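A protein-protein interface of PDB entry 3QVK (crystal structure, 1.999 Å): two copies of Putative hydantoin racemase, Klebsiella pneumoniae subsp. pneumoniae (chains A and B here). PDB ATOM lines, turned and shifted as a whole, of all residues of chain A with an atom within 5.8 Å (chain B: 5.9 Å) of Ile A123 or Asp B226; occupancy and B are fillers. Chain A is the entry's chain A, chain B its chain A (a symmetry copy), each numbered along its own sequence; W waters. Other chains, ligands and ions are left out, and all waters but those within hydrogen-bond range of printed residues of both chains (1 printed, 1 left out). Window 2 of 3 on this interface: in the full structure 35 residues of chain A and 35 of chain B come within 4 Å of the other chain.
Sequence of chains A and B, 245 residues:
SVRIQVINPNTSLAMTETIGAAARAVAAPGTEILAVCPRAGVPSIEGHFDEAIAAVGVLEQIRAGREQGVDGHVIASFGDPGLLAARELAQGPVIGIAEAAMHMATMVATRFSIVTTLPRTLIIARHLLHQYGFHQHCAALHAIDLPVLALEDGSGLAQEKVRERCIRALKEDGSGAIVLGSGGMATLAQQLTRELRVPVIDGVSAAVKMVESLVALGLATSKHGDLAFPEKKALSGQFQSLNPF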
ATOM      1  N   HIS A  48      -5.785 -34.169 -12.777  1.00  0.00           N
ATOM      2  CA  HIS A  48      -6.271 -35.485 -13.194  1.00  0.00           C
ATOM      3  C   HIS A  48      -5.276 -36.611 -12.916  1.00  0.00           C
ATOM      4  O   HIS A  48      -5.677 -37.724 -12.565  1.00  0.00           O
ATOM      5  CB  HIS A  48      -6.655 -35.459 -14.677  1.00  0.00           C
ATOM      6  CG  HIS A  48      -7.607 -34.359 -15.031  1.00  0.00           C
ATOM      7  ND1 HIS A  48      -7.186 -33.116 -15.452  1.00  0.00           N
ATOM      8  CD2 HIS A  48      -8.960 -34.314 -15.020  1.00  0.00           C
ATOM      9  CE1 HIS A  48      -8.239 -32.353 -15.689  1.00  0.00           C
ATOM     10  NE2 HIS A  48      -9.327 -33.057 -15.436  1.00  0.00           N
ATOM     11  N   PRO A 119      -7.137 -23.054  -9.748  1.00  0.00           N
ATOM     12  CA  PRO A 119      -7.901 -22.910 -10.991  1.00  0.00           C
ATOM     13  C   PRO A 119      -8.016 -24.200 -11.809  1.00  0.00           C
ATOM     14  O   PRO A 119      -9.061 -24.448 -12.408  1.00  0.00           O
ATOM     15  CB  PRO A 119      -7.104 -21.861 -11.769  1.00  0.00           C
ATOM     16  CG  PRO A 119      -6.487 -21.023 -10.717  1.00  0.00           C
ATOM     17  CD  PRO A 119      -6.148 -21.967  -9.596  1.00  0.00           C
ATOM     18  N   ARG A 120      -6.961 -25.013 -11.824  1.00  0.00           N
ATOM     19  CA  ARG A 120      -6.951 -26.245 -12.623  1.00  0.00           C
ATOM     20  C   ARG A 120      -7.841 -27.367 -12.065  1.00  0.00           C
ATOM     21  O   ARG A 120      -8.084 -28.364 -12.749  1.00  0.00           O
ATOM     22  CB  ARG A 120      -5.518 -26.741 -12.865  1.00  0.00           C
ATOM     23  CG  ARG A 120      -4.802 -27.311 -11.643  1.00  0.00           C
ATOM     24  CD  ARG A 120      -3.438 -27.879 -12.027  1.00  0.00           C
ATOM     25  NE  ARG A 120      -3.536 -28.884 -13.087  1.00  0.00           N
ATOM     26  CZ  ARG A 120      -2.497 -29.426 -13.720  1.00  0.00           C
ATOM     27  NH1 ARG A 120      -1.255 -29.075 -13.409  1.00  0.00           N
ATOM     28  NH2 ARG A 120      -2.702 -30.326 -14.671  1.00  0.00           N
ATOM     29  N   THR A 121      -8.322 -27.201 -10.834  1.00  0.00           N
ATOM     30  CA  THR A 121      -9.240 -28.172 -10.230  1.00  0.00           C
ATOM     31  C   THR A 121     -10.704 -27.840 -10.533  1.00  0.00           C
ATOM     32  O   THR A 121     -11.589 -28.666 -10.305  1.00  0.00           O
ATOM     33  CB  THR A 121      -9.040 -28.308  -8.696  1.00  0.00           C
ATOM     34  OG1 THR A 121      -9.366 -27.072  -8.048  1.00  0.00           O
ATOM     35  CG2 THR A 121      -7.602 -28.698  -8.365  1.00  0.00           C
ATOM     36  N   LEU A 122     -10.945 -26.635 -11.051  1.00  0.00           N
ATOM     37  CA  LEU A 122     -12.302 -26.177 -11.375  1.00  0.00           C
ATOM     38  C   LEU A 122     -13.006 -27.083 -12.386  1.00  0.00           C
ATOM     39  O   LEU A 122     -14.182 -27.404 -12.213  1.00  0.00           O
ATOM     40  CB  LEU A 122     -12.292 -24.727 -11.874  1.00  0.00           C
ATOM     41  CG  LEU A 122     -12.016 -23.608 -10.863  1.00  0.00           C
ATOM     42  CD1 LEU A 122     -11.684 -22.310 -11.581  1.00  0.00           C
ATOM     43  CD2 LEU A 122     -13.191 -23.408  -9.914  1.00  0.00           C
ATOM     44  N   ILE A 123     -12.278 -27.496 -13.425  1.00  0.00           N
ATOM     45  CA  ILE A 123     -12.809 -28.404 -14.450  1.00  0.00           C
ATOM     46  C   ILE A 123     -13.255 -29.748 -13.860  1.00  0.00           C
ATOM     47  O   ILE A 123     -14.234 -30.339 -14.320  1.00  0.00           O
ATOM     48  CB  ILE A 123     -11.807 -28.611 -15.634  1.00  0.00           C
ATOM     49  CG1 ILE A 123     -12.472 -29.342 -16.813  1.00  0.00           C
ATOM     50  CG2 ILE A 123     -10.539 -29.342 -15.181  1.00  0.00           C
ATOM     51  CD1 ILE A 123     -13.491 -28.510 -17.581  1.00  0.00           C
ATOM     52  N   ILE A 124     -12.531 -30.215 -12.842  1.00  0.00           N
ATOM     53  CA  ILE A 124     -12.875 -31.450 -12.137  1.00  0.00           C
ATOM     54  C   ILE A 124     -14.196 -31.273 -11.384  1.00  0.00           C
ATOM     55  O   ILE A 124     -15.061 -32.153 -11.421  1.00  0.00           O
ATOM     56  CB  ILE A 124     -11.737 -31.894 -11.178  1.00  0.00           C
ATOM     57  CG1 ILE A 124     -10.492 -32.296 -11.983  1.00  0.00           C
ATOM     58  CG2 ILE A 124     -12.198 -33.042 -10.277  1.00  0.00           C
ATOM     59  CD1 ILE A 124      -9.214 -32.409 -11.160  1.00  0.00           C
ATOM     60  N   ALA A 125     -14.347 -30.127 -10.724  1.00  0.00           N
ATOM     61  CA  ALA A 125     -15.585 -29.776 -10.032  1.00  0.00           C
ATOM     62  C   ALA A 125     -16.753 -29.604 -11.008  1.00  0.00           C
ATOM     63  O   ALA A 125     -17.881 -29.983 -10.693  1.00  0.00           O
ATOM     64  CB  ALA A 125     -15.394 -28.522  -9.195  1.00  0.00           C
ATOM     65  N   ARG A 126     -16.470 -29.042 -12.186  1.00  0.00           N
ATOM     66  CA  ARG A 126     -17.477 -28.873 -13.242  1.00  0.00           C
ATOM     67  C   ARG A 126     -17.987 -30.219 -13.751  1.00  0.00           C
ATOM     68  O   ARG A 126     -19.188 -30.385 -13.978  1.00  0.00           O
ATOM     69  CB  ARG A 126     -16.922 -28.057 -14.416  1.00  0.00           C
ATOM     70  CG  ARG A 126     -16.702 -26.580 -14.126  1.00  0.00           C
ATOM     71  CD  ARG A 126     -16.175 -25.851 -15.362  1.00  0.00           C
ATOM     72  NE  ARG A 126     -15.418 -24.650 -15.010  1.00  0.00           N
ATOM     73  CZ  ARG A 126     -15.941 -23.434 -14.870  1.00  0.00           C
ATOM     74  NH1 ARG A 126     -15.159 -22.413 -14.544  1.00  0.00           N
ATOM     75  NH2 ARG A 126     -17.241 -23.232 -15.053  1.00  0.00           N
ATOM     76  N   HIS A 127     -17.066 -31.167 -13.926  1.00  0.00           N
ATOM     77  CA  HIS A 127     -17.402 -32.517 -14.371  1.00  0.00           C
ATOM     78  C   HIS A 127     -18.276 -33.239 -13.347  1.00  0.00           C
ATOM     79  O   HIS A 127     -19.232 -33.925 -13.718  1.00  0.00           O
ATOM     80  CB  HIS A 127     -16.131 -33.326 -14.655  1.00  0.00           C
ATOM     81  CG  HIS A 127     -16.392 -34.759 -15.006  1.00  0.00           C
ATOM     82  ND1 HIS A 127     -16.334 -35.775 -14.076  1.00  0.00           N
ATOM     83  CD2 HIS A 127     -16.723 -35.344 -16.181  1.00  0.00           C
ATOM     84  CE1 HIS A 127     -16.611 -36.925 -14.664  1.00  0.00           C
ATOM     85  NE2 HIS A 127     -16.851 -36.691 -15.942  1.00  0.00           N
ATOM     86  N   LEU A 128     -17.946 -33.079 -12.065  1.00  0.00           N
ATOM     87  CA  LEU A 128     -18.723 -33.683 -10.980  1.00  0.00           C
ATOM     88  C   LEU A 128     -20.132 -33.101 -10.888  1.00  0.00           C
ATOM     89  O   LEU A 128     -21.086 -33.826 -10.602  1.00  0.00           O
ATOM     90  CB  LEU A 128     -18.004 -33.538  -9.635  1.00  0.00           C
ATOM     91  CG  LEU A 128     -16.755 -34.388  -9.373  1.00  0.00           C
ATOM     92  CD1 LEU A 128     -16.163 -34.021  -8.029  1.00  0.00           C
ATOM     93  CD2 LEU A 128     -17.053 -35.884  -9.430  1.00  0.00           C
ATOM     94  N   GLU B  88      -2.218 -34.871 -19.220  1.00  0.00           N
ATOM     95  CA  GLU B  88      -1.390 -34.049 -18.342  1.00  0.00           C
ATOM     96  C   GLU B  88       0.071 -34.493 -18.379  1.00  0.00           C
ATOM     97  O   GLU B  88       0.973 -33.661 -18.491  1.00  0.00           O
ATOM     98  CB  GLU B  88      -1.908 -34.095 -16.903  1.00  0.00           C
ATOM     99  CG  GLU B  88      -3.215 -33.347 -16.680  1.00  0.00           C
ATOM    100  CD  GLU B  88      -3.633 -33.305 -15.221  1.00  0.00           C
ATOM    101  OE1 GLU B  88      -2.964 -33.937 -14.379  1.00  0.00           O
ATOM    102  OE2 GLU B  88      -4.633 -32.627 -14.911  1.00  0.00           O
ATOM    103  N   SER B 222      -2.756 -29.111 -25.014  1.00  0.00           N
ATOM    104  CA  SER B 222      -2.533 -27.796 -24.427  1.00  0.00           C
ATOM    105  C   SER B 222      -1.952 -27.920 -23.023  1.00  0.00           C
ATOM    106  O   SER B 222      -2.521 -28.597 -22.163  1.00  0.00           O
ATOM    107  CB  SER B 222      -3.839 -27.003 -24.373  1.00  0.00           C
ATOM    108  OG  SER B 222      -3.626 -25.724 -23.803  1.00  0.00           O
ATOM    109  N   HIS B 224      -1.559 -25.293 -21.194  1.00  0.00           N
ATOM    110  CA  HIS B 224      -2.068 -24.088 -20.564  1.00  0.00           C
ATOM    111  C   HIS B 224      -3.340 -24.421 -19.789  1.00  0.00           C
ATOM    112  O   HIS B 224      -4.385 -24.707 -20.381  1.00  0.00           O
ATOM    113  CB  HIS B 224      -2.340 -23.020 -21.628  1.00  0.00           C
ATOM    114  CG  HIS B 224      -3.017 -21.793 -21.106  1.00  0.00           C
ATOM    115  ND1 HIS B 224      -4.381 -21.608 -21.180  1.00  0.00           N
ATOM    116  CD2 HIS B 224      -2.519 -20.681 -20.514  1.00  0.00           C
ATOM    117  CE1 HIS B 224      -4.694 -20.439 -20.650  1.00  0.00           C
ATOM    118  NE2 HIS B 224      -3.582 -19.857 -20.239  1.00  0.00           N
ATOM    119  N   GLY B 225      -3.235 -24.403 -18.464  1.00  0.00           N
ATOM    120  CA  GLY B 225      -4.386 -24.616 -17.594  1.00  0.00           C
ATOM    121  C   GLY B 225      -4.643 -26.055 -17.180  1.00  0.00           C
ATOM    122  O   GLY B 225      -3.841 -26.657 -16.464  1.00  0.00           O
ATOM    123  N   ASP B 226      -5.766 -26.598 -17.646  1.00  0.00           N
ATOM    124  CA  ASP B 226      -6.305 -27.869 -17.150  1.00  0.00           C
ATOM    125  C   ASP B 226      -5.457 -29.103 -17.452  1.00  0.00           C
ATOM    126  O   ASP B 226      -5.384 -30.023 -16.635  1.00  0.00           O
ATOM    127  CB  ASP B 226      -7.729 -28.085 -17.676  1.00  0.00           C
ATOM    128  CG  ASP B 226      -8.702 -27.017 -17.207  1.00  0.00           C
ATOM    129  OD1 ASP B 226      -8.361 -26.235 -16.290  1.00  0.00           O
ATOM    130  OD2 ASP B 226      -9.820 -26.965 -17.759  1.00  0.00           O
ATOM    131  N   LEU B 227      -4.835 -29.127 -18.628  1.00  0.00           N
ATOM    132  CA  LEU B 227      -4.053 -30.289 -19.044  1.00  0.00           C
ATOM    133  C   LEU B 227      -2.550 -30.012 -19.023  1.00  0.00           C
ATOM    134  O   LEU B 227      -1.771 -30.665 -19.723  1.00  0.00           O
ATOM    135  CB  LEU B 227      -4.519 -30.799 -20.414  1.00  0.00           C
ATOM    136  CG  LEU B 227      -5.982 -31.248 -20.548  1.00  0.00           C
ATOM    137  CD1 LEU B 227      -6.290 -31.648 -21.981  1.00  0.00           C
ATOM    138  CD2 LEU B 227      -6.331 -32.387 -19.590  1.00  0.00           C
ATOM    139  N   ALA B 228      -2.157 -29.041 -18.200  1.00  0.00           N
ATOM    140  CA  ALA B 228      -0.751 -28.744 -17.949  1.00  0.00           C
ATOM    141  C   ALA B 228      -0.087 -29.933 -17.264  1.00  0.00           C
ATOM    142  O   ALA B 228      -0.767 -30.766 -16.653  1.00  0.00           O
ATOM    143  CB  ALA B 228      -0.622 -27.499 -17.087  1.00  0.00           C
HETATM  144  O   HOH W   1     -10.264 -25.645 -14.435  1.00  0.00           O
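ND1 of His A48 lies within hydrogen-bond range of OE2 of Glu B88 (2.7 Å). The backbone carbonyl oxygen (O) of Ala B228 sits at hydrogen-bond distance from the guanidinium group (NH2) of Arg A120 (2.8 Å). NH2 of Arg A120 lies within hydrogen-bond range of O of Asp B226, 3.3 Å away. The guanidinium group (NH2) of Arg A120 lies within salt-bridge range of the side-chain carboxylate (OE2) of Glu B88 (3.0 Å).
Among the printed residues, merely in contact across the chains: Ile A123 with Asp B226 (3.3 Å), His A48 with Asp B226 (3.8 Å) and Arg A120 with Gly B225 (3.97 Å).
Ile A123 touches just one residue of chain B: Asp B226. Asp B226 touches just these residues of chain A: His A48, Arg A120 and Ile A123. Printed residues of chain B within 4 Å of His A48: Glu B88 and Asp B226. Of the printed residues of chain A, Gly B225 touches Arg A120. Of the printed residues of chain B, Arg A120 touches Glu B88 (3.0 Å), Gly B225 (3.97 Å), Asp B226 (3.3 Å) and Ala B228 (2.8 Å). Of the printed residues of chain A, Ala B228 touches Arg A120 (2.8 Å).
Of the 11 printed residues of chain A, 3 touch a printed residue of chain B. Hydrophobic or aromatic side chains of chain A that line the printed part of chain B: His A48 and Ile A123. Among the printed residues, 7 pairs touch across the chains.
No position is printed for both chains.
Water W1 lies within hydrogen-bond range of O of Pro A119 (2.6 Å), OD1 of Asp B226 (2.7 Å) and N of Ile A123 (2.9 Å).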
